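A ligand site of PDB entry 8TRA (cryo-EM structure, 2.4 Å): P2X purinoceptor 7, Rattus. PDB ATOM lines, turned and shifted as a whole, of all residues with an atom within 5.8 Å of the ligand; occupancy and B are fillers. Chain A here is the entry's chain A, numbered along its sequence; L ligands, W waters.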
ATOM      1  N   GLU A 495      15.953  -1.266  17.824  1.00  0.00           N
ATOM      2  CA  GLU A 495      16.756  -0.505  16.869  1.00  0.00           C
ATOM      3  C   GLU A 495      17.541  -1.393  15.916  1.00  0.00           C
ATOM      4  O   GLU A 495      18.272  -0.860  15.073  1.00  0.00           O
ATOM      5  CB  GLU A 495      17.701   0.439  17.612  1.00  0.00           C
ATOM      6  CG  GLU A 495      16.997   1.501  18.436  1.00  0.00           C
ATOM      7  CD  GLU A 495      17.933   2.630  18.849  1.00  0.00           C
ATOM      8  OE1 GLU A 495      19.114   2.591  18.457  1.00  0.00           O
ATOM      9  OE2 GLU A 495      17.474   3.541  19.559  1.00  0.00           O
ATOM     10  N   SER A 543      18.600  19.165  19.185  1.00  0.00           N
ATOM     11  CA  SER A 543      17.621  18.147  19.558  1.00  0.00           C
ATOM     12  C   SER A 543      16.306  18.349  18.808  1.00  0.00           C
ATOM     13  O   SER A 543      15.690  17.386  18.328  1.00  0.00           O
ATOM     14  CB  SER A 543      17.387  18.176  21.068  1.00  0.00           C
ATOM     15  OG  SER A 543      16.886  19.432  21.475  1.00  0.00           O
ATOM     16  N   ARG A 546      16.819  17.119  15.288  1.00  0.00           N
ATOM     17  CA  ARG A 546      16.831  15.663  15.231  1.00  0.00           C
ATOM     18  C   ARG A 546      15.415  15.102  15.312  1.00  0.00           C
ATOM     19  O   ARG A 546      15.059  14.191  14.559  1.00  0.00           O
ATOM     20  CB  ARG A 546      17.706  15.099  16.359  1.00  0.00           C
ATOM     21  CG  ARG A 546      18.548  13.898  15.958  1.00  0.00           C
ATOM     22  CD  ARG A 546      19.500  13.477  17.071  1.00  0.00           C
ATOM     23  NE  ARG A 546      19.011  13.829  18.397  1.00  0.00           N
ATOM     24  CZ  ARG A 546      19.469  14.836  19.136  1.00  0.00           C
ATOM     25  NH1 ARG A 546      20.444  15.627  18.709  1.00  0.00           N
ATOM     26  NH2 ARG A 546      18.945  15.050  20.337  1.00  0.00           N
ATOM     27  N   HIS A 547      14.609  15.628  16.235  1.00  0.00           N
ATOM     28  CA  HIS A 547      13.227  15.181  16.336  1.00  0.00           C
ATOM     29  C   HIS A 547      12.443  15.495  15.071  1.00  0.00           C
ATOM     30  O   HIS A 547      11.650  14.675  14.606  1.00  0.00           O
ATOM     31  CB  HIS A 547      12.558  15.827  17.553  1.00  0.00           C
ATOM     32  CG  HIS A 547      13.248  15.539  18.854  1.00  0.00           C
ATOM     33  ND1 HIS A 547      12.888  16.144  20.033  1.00  0.00           N
ATOM     34  CD2 HIS A 547      14.282  14.714  19.148  1.00  0.00           C
ATOM     35  CE1 HIS A 547      13.665  15.702  21.011  1.00  0.00           C
ATOM     36  NE2 HIS A 547      14.515  14.828  20.497  1.00  0.00           N
ATOM     37  N   TYR A 550      13.400  12.944  12.457  1.00  0.00           N
ATOM     38  CA  TYR A 550      12.700  11.702  12.707  1.00  0.00           C
ATOM     39  C   TYR A 550      11.253  11.781  12.215  1.00  0.00           C
ATOM     40  O   TYR A 550      10.756  10.881  11.538  1.00  0.00           O
ATOM     41  CB  TYR A 550      12.726  11.355  14.196  1.00  0.00           C
ATOM     42  CG  TYR A 550      14.110  11.124  14.776  1.00  0.00           C
ATOM     43  CD1 TYR A 550      15.143  10.623  14.000  1.00  0.00           C
ATOM     44  CD2 TYR A 550      14.371  11.387  16.114  1.00  0.00           C
ATOM     45  CE1 TYR A 550      16.399  10.408  14.533  1.00  0.00           C
ATOM     46  CE2 TYR A 550      15.628  11.177  16.655  1.00  0.00           C
ATOM     47  CZ  TYR A 550      16.625  10.680  15.860  1.00  0.00           C
ATOM     48  OH  TYR A 550      17.882  10.470  16.401  1.00  0.00           O
ATOM     49  N   ALA A 554       9.471   9.639   9.196  1.00  0.00           N
ATOM     50  CA  ALA A 554       8.299   8.827   9.491  1.00  0.00           C
ATOM     51  C   ALA A 554       7.119   9.214   8.611  1.00  0.00           C
ATOM     52  O   ALA A 554       6.417   8.352   8.084  1.00  0.00           O
ATOM     53  CB  ALA A 554       7.928   8.955  10.977  1.00  0.00           C
ATOM     54  N   ALA A 564       2.950   6.936  11.665  1.00  0.00           N
ATOM     55  CA  ALA A 564       4.230   7.601  11.850  1.00  0.00           C
ATOM     56  C   ALA A 564       4.601   7.704  13.323  1.00  0.00           C
ATOM     57  O   ALA A 564       5.762   7.504  13.698  1.00  0.00           O
ATOM     58  CB  ALA A 564       4.199   8.984  11.215  1.00  0.00           C
ATOM     59  N   ASP A 565       3.625   8.007  14.183  1.00  0.00           N
ATOM     60  CA  ASP A 565       3.896   8.118  15.609  1.00  0.00           C
ATOM     61  C   ASP A 565       4.396   6.817  16.213  1.00  0.00           C
ATOM     62  O   ASP A 565       5.074   6.846  17.246  1.00  0.00           O
ATOM     63  CB  ASP A 565       2.643   8.585  16.346  1.00  0.00           C
ATOM     64  CG  ASP A 565       2.276  10.019  16.041  1.00  0.00           C
ATOM     65  OD1 ASP A 565       3.160  10.770  15.559  1.00  0.00           O
ATOM     66  OD2 ASP A 565       1.108  10.405  16.273  1.00  0.00           O
ATOM     67  N   PHE A 566       4.084   5.679  15.587  1.00  0.00           N
ATOM     68  CA  PHE A 566       4.530   4.374  16.073  1.00  0.00           C
ATOM     69  C   PHE A 566       5.540   3.729  15.140  1.00  0.00           C
ATOM     70  O   PHE A 566       5.885   2.552  15.321  1.00  0.00           O
ATOM     71  CB  PHE A 566       3.329   3.451  16.262  1.00  0.00           C
ATOM     72  CG  PHE A 566       2.546   3.735  17.512  1.00  0.00           C
ATOM     73  CD1 PHE A 566       2.961   3.243  18.731  1.00  0.00           C
ATOM     74  CD2 PHE A 566       1.388   4.500  17.460  1.00  0.00           C
ATOM     75  CE1 PHE A 566       2.243   3.501  19.880  1.00  0.00           C
ATOM     76  CE2 PHE A 566       0.672   4.770  18.601  1.00  0.00           C
ATOM     77  CZ  PHE A 566       1.107   4.268  19.823  1.00  0.00           C
ATOM     78  N   ALA A 567       6.045   4.462  14.145  1.00  0.00           N
ATOM     79  CA  ALA A 567       7.042   3.914  13.239  1.00  0.00           C
ATOM     80  C   ALA A 567       8.366   3.722  13.969  1.00  0.00           C
ATOM     81  O   ALA A 567       8.596   4.247  15.065  1.00  0.00           O
ATOM     82  CB  ALA A 567       7.230   4.832  12.034  1.00  0.00           C
ATOM     83  N   ILE A 568       9.259   2.947  13.344  1.00  0.00           N
ATOM     84  CA  ILE A 568      10.593   2.696  13.873  1.00  0.00           C
ATOM     85  C   ILE A 568      11.587   3.047  12.765  1.00  0.00           C
ATOM     86  O   ILE A 568      11.522   2.484  11.666  1.00  0.00           O
ATOM     87  CB  ILE A 568      10.770   1.243  14.326  1.00  0.00           C
ATOM     88  CG1 ILE A 568       9.668   0.842  15.304  1.00  0.00           C
ATOM     89  CG2 ILE A 568      12.143   1.053  14.953  1.00  0.00           C
ATOM     90  CD1 ILE A 568       9.696   1.601  16.622  1.00  0.00           C
ATOM     91  N   LEU A 569      12.504   3.951  13.067  1.00  0.00           N
ATOM     92  CA  LEU A 569      13.480   4.371  12.075  1.00  0.00           C
ATOM     93  C   LEU A 569      14.534   3.278  11.880  1.00  0.00           C
ATOM     94  O   LEU A 569      14.926   2.625  12.846  1.00  0.00           O
ATOM     95  CB  LEU A 569      14.153   5.676  12.485  1.00  0.00           C
ATOM     96  CG  LEU A 569      13.628   6.940  11.812  1.00  0.00           C
ATOM     97  CD1 LEU A 569      12.358   7.433  12.491  1.00  0.00           C
ATOM     98  CD2 LEU A 569      14.689   8.021  11.811  1.00  0.00           C
ATOM     99  N   PRO A 570      15.016   3.075  10.654  1.00  0.00           N
ATOM    100  CA  PRO A 570      16.148   2.160  10.459  1.00  0.00           C
ATOM    101  C   PRO A 570      17.403   2.703  11.131  1.00  0.00           C
ATOM    102  O   PRO A 570      17.569   3.911  11.317  1.00  0.00           O
ATOM    103  CB  PRO A 570      16.307   2.096   8.935  1.00  0.00           C
ATOM    104  CG  PRO A 570      15.001   2.562   8.392  1.00  0.00           C
ATOM    105  CD  PRO A 570      14.480   3.552   9.370  1.00  0.00           C
ATOM    106  N   ARG A 574      18.617   6.551  11.253  1.00  0.00           N
ATOM    107  CA  ARG A 574      18.698   7.099  12.605  1.00  0.00           C
ATOM    108  C   ARG A 574      20.090   7.642  12.891  1.00  0.00           C
ATOM    109  O   ARG A 574      20.246   8.780  13.367  1.00  0.00           O
ATOM    110  CB  ARG A 574      18.309   6.022  13.621  1.00  0.00           C
ATOM    111  CG  ARG A 574      18.470   6.401  15.083  1.00  0.00           C
ATOM    112  CD  ARG A 574      18.541   5.164  15.965  1.00  0.00           C
ATOM    113  NE  ARG A 574      17.470   4.225  15.661  1.00  0.00           N
ATOM    114  CZ  ARG A 574      16.197   4.404  15.986  1.00  0.00           C
ATOM    115  NH1 ARG A 574      15.791   5.484  16.634  1.00  0.00           N
ATOM    116  NH2 ARG A 574      15.309   3.471  15.661  1.00  0.00           N
ATOM    117  N   ARG A 578      21.504  11.428  13.499  1.00  0.00           N
ATOM    118  CA  ARG A 578      22.265  11.790  14.685  1.00  0.00           C
ATOM    119  C   ARG A 578      23.644  12.344  14.334  1.00  0.00           C
ATOM    120  O   ARG A 578      24.149  13.249  15.008  1.00  0.00           O
ATOM    121  CB  ARG A 578      22.394  10.578  15.614  1.00  0.00           C
ATOM    122  CG  ARG A 578      21.140  10.325  16.436  1.00  0.00           C
ATOM    123  CD  ARG A 578      21.006   8.877  16.855  1.00  0.00           C
ATOM    124  NE  ARG A 578      19.788   8.655  17.630  1.00  0.00           N
ATOM    125  CZ  ARG A 578      19.518   7.538  18.286  1.00  0.00           C
ATOM    126  NH1 ARG A 578      20.353   6.513  18.298  1.00  0.00           N
ATOM    127  NH2 ARG A 578      18.366   7.450  18.960  1.00  0.00           N
ATOM    128  N   LYS A 583      24.376  14.648  19.561  1.00  0.00           N
ATOM    129  CA  LYS A 583      24.179  15.058  20.946  1.00  0.00           C
ATOM    130  C   LYS A 583      25.533  15.124  21.637  1.00  0.00           C
ATOM    131  O   LYS A 583      26.302  14.164  21.609  1.00  0.00           O
ATOM    132  CB  LYS A 583      23.255  14.085  21.670  1.00  0.00           C
ATOM    133  CG  LYS A 583      22.663  14.619  22.952  1.00  0.00           C
ATOM    134  CD  LYS A 583      21.873  13.537  23.684  1.00  0.00           C
ATOM    135  CE  LYS A 583      20.989  14.119  24.763  1.00  0.00           C
ATOM    136  NZ  LYS A 583      20.134  13.076  25.400  1.00  0.00           N
ATOM    137  N   GLN A 587      23.060  10.516  26.176  1.00  0.00           N
ATOM    138  CA  GLN A 587      22.747   9.214  25.600  1.00  0.00           C
ATOM    139  C   GLN A 587      21.358   9.272  24.972  1.00  0.00           C
ATOM    140  O   GLN A 587      20.412   9.792  25.592  1.00  0.00           O
ATOM    141  CB  GLN A 587      22.803   8.112  26.652  1.00  0.00           C
ATOM    142  CG  GLN A 587      23.337   6.790  26.137  1.00  0.00           C
ATOM    143  CD  GLN A 587      24.852   6.751  26.066  1.00  0.00           C
ATOM    144  OE1 GLN A 587      25.529   7.665  26.519  1.00  0.00           O
ATOM    145  NE2 GLN A 587      25.390   5.670  25.491  1.00  0.00           N
ATOM    146  N   TYR A 588      21.227   8.750  23.753  1.00  0.00           N
ATOM    147  CA  TYR A 588      19.962   8.819  23.039  1.00  0.00           C
ATOM    148  C   TYR A 588      18.937   7.889  23.672  1.00  0.00           C
ATOM    149  O   TYR A 588      19.220   6.716  23.932  1.00  0.00           O
ATOM    150  CB  TYR A 588      20.174   8.448  21.570  1.00  0.00           C
ATOM    151  CG  TYR A 588      21.093   9.398  20.837  1.00  0.00           C
ATOM    152  CD1 TYR A 588      20.703  10.704  20.575  1.00  0.00           C
ATOM    153  CD2 TYR A 588      22.353   8.992  20.414  1.00  0.00           C
ATOM    154  CE1 TYR A 588      21.546  11.573  19.902  1.00  0.00           C
ATOM    155  CE2 TYR A 588      23.201   9.854  19.744  1.00  0.00           C
ATOM    156  CZ  TYR A 588      22.786  11.141  19.486  1.00  0.00           C
ATOM    157  OH  TYR A 588      23.622  12.011  18.825  1.00  0.00           O
ATOM    158  N   SER A 589      17.741   8.428  23.936  1.00  0.00           N
ATOM    159  CA  SER A 589      16.675   7.635  24.530  1.00  0.00           C
ATOM    160  C   SER A 589      16.017   6.700  23.524  1.00  0.00           C
ATOM    161  O   SER A 589      15.521   5.637  23.915  1.00  0.00           O
ATOM    162  CB  SER A 589      15.628   8.560  25.152  1.00  0.00           C
ATOM    163  OG  SER A 589      14.970   9.320  24.154  1.00  0.00           O
ATOM    164  N   GLY A 590      16.002   7.077  22.249  1.00  0.00           N
ATOM    165  CA  GLY A 590      15.357   6.258  21.243  1.00  0.00           C
ATOM    166  C   GLY A 590      13.846   6.481  21.216  1.00  0.00           C
ATOM    167  O   GLY A 590      13.316   7.482  21.720  1.00  0.00           O
ATOM    168  N   PHE A 591      13.157   5.526  20.614  1.00  0.00           N
ATOM    169  CA  PHE A 591      11.707   5.617  20.492  1.00  0.00           C
ATOM    170  C   PHE A 591      11.054   5.605  21.871  1.00  0.00           C
ATOM    171  O   PHE A 591      11.456   4.843  22.759  1.00  0.00           O
ATOM    172  CB  PHE A 591      11.167   4.459  19.645  1.00  0.00           C
ATOM    173  CG  PHE A 591       9.671   4.370  19.612  1.00  0.00           C
ATOM    174  CD1 PHE A 591       8.930   5.306  18.922  1.00  0.00           C
ATOM    175  CD2 PHE A 591       9.012   3.356  20.283  1.00  0.00           C
ATOM    176  CE1 PHE A 591       7.546   5.232  18.886  1.00  0.00           C
ATOM    177  CE2 PHE A 591       7.635   3.280  20.259  1.00  0.00           C
ATOM    178  CZ  PHE A 591       6.901   4.215  19.556  1.00  0.00           C
ATOM    179  N   LYS A 592      10.036   6.447  22.044  1.00  0.00           N
ATOM    180  CA  LYS A 592       9.298   6.549  23.288  1.00  0.00           C
ATOM    181  C   LYS A 592       7.818   6.371  23.012  1.00  0.00           C
ATOM    182  O   LYS A 592       7.289   6.881  22.012  1.00  0.00           O
ATOM    183  CB  LYS A 592       9.546   7.906  23.971  1.00  0.00           C
ATOM    184  CG  LYS A 592       9.005   7.996  25.389  1.00  0.00           C
ATOM    185  CD  LYS A 592       8.677   9.432  25.792  1.00  0.00           C
ATOM    186  CE  LYS A 592       7.399   9.506  26.612  1.00  0.00           C
ATOM    187  NZ  LYS A 592       6.184   9.496  25.761  1.00  0.00           N
HETATM  188  P1  LIG L   1      17.377  12.211  22.842  1.00  0.00           P
HETATM  189  O1  LIG L   1      18.613  12.799  22.224  1.00  0.00           O
HETATM  190  O2  LIG L   1      16.232  13.192  22.719  1.00  0.00           O
HETATM  191  O3  LIG L   1      17.623  11.933  24.302  1.00  0.00           O
HETATM  192  O4  LIG L   1      16.991  10.829  22.125  1.00  0.00           O
HETATM  193  P2  LIG L   1      16.575  10.761  20.568  1.00  0.00           P
HETATM  194  O5  LIG L   1      17.531  11.545  19.704  1.00  0.00           O
HETATM  195  O6  LIG L   1      16.525   9.329  20.120  1.00  0.00           O
HETATM  196  O7  LIG L   1      15.115  11.412  20.551  1.00  0.00           O
HETATM  197  C1  LIG L   1      14.075  10.809  21.310  1.00  0.00           C
HETATM  198  C2  LIG L   1      12.726  11.186  20.733  1.00  0.00           C
HETATM  199  O8  LIG L   1      12.731  10.919  19.331  1.00  0.00           O
HETATM  200  C3  LIG L   1      11.612  10.373  21.359  1.00  0.00           C
HETATM  201  O9  LIG L   1      10.579  11.213  21.864  1.00  0.00           O
HETATM  202  C4  LIG L   1      11.084   9.472  20.276  1.00  0.00           C
HETATM  203  O10 LIG L   1       9.657   9.499  20.211  1.00  0.00           O
HETATM  204  C5  LIG L   1      11.716   9.976  18.985  1.00  0.00           C
HETATM  205  N1  LIG L   1      12.308   8.825  18.290  1.00  0.00           N
HETATM  206  C6  LIG L   1      13.575   8.390  18.422  1.00  0.00           C
HETATM  207  N2  LIG L   1      13.780   7.301  17.648  1.00  0.00           N
HETATM  208  C7  LIG L   1      12.632   7.028  17.011  1.00  0.00           C
HETATM  209  C8  LIG L   1      12.167   6.015  16.043  1.00  0.00           C
HETATM  210  O11 LIG L   1      12.943   5.122  15.635  1.00  0.00           O
HETATM  211  N3  LIG L   1      10.907   6.076  15.614  1.00  0.00           N
HETATM  212  C9  LIG L   1      10.056   7.015  16.043  1.00  0.00           C
HETATM  213  N4  LIG L   1       8.780   7.017  15.569  1.00  0.00           N
HETATM  214  N5  LIG L   1      10.406   7.983  16.927  1.00  0.00           N
HETATM  215  C10 LIG L   1      11.658   8.032  17.433  1.00  0.00           C
HETATM  216  O   HOH W   1       9.253  10.831  15.715  1.00  0.00           O
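OH of Tyr 588 sits at hydrogen-bond distance from N of Lys 583, 2.8 Å away.
The backbone carbonyl oxygen (O) of Leu 569 is in hydrogen-bond range of the guanidinium group (NH2) of Arg 574, at 3.0 Å.
The guanidinium group (NE) of Arg 578 is in hydrogen-bond range of the side-chain hydroxyl (OH) of Tyr 550 (2.9 Å).
The side-chain amino group of Lys 583 is in hydrogen-bond range of the backbone carbonyl oxygen of Gln 587.
OE1 of Glu 495 is in salt-bridge range of NE of Arg 574 (3.6 Å).
Residues that only touch the ligand: Ala 564 (3.6 Å), Ile 568 (3.8 Å), Gln 587 (3.7 Å), Tyr 588 (3.4 Å), Phe 591 (3.5 Å) and Lys 592 (3.6 Å).
Hydrophobic or aromatic side chains that line the ligand: His 547, Tyr 550, Leu 569, Tyr 588 and Phe 591.
Of the 22 residues printed, 16 come within 4 Å of the ligand.
The side-chain amino group (NZ) of Lys 583 lies within salt-bridge range of an oxygen (O3) of the ligand (3.0 Å).
An oxygen (O1) of the ligand lies within salt-bridge range of the guanidinium group (NH2) of Arg 546, 3.0 Å away.
An oxygen (O4) of the ligand sits at hydrogen-bond distance from the backbone NH (N) of Ser 589, at 3.1 Å.
An oxygen (O2) of the ligand lies within hydrogen-bond range of a ring nitrogen (NE2) of His 547, at 3.2 Å.
O of Ala 567 sits at hydrogen-bond distance from N4 of the ligand, at 2.8 Å.
The backbone NH of Gly 590 sits at hydrogen-bond distance from an oxygen (O6) of the ligand.
NH2 of Arg 574 is in hydrogen-bond range of O11 of the ligand.
NH2 of Arg 578 lies within salt-bridge range of O6 of the ligand (2.9 Å).
O5 of the ligand lies within hydrogen-bond range of OH of Tyr 550 (3.5 Å).
O11 of the ligand lies within hydrogen-bond range of N of Leu 569.
The side-chain hydroxyl (OG) of Ser 589 is in hydrogen-bond range of an oxygen (O4) of the ligand.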
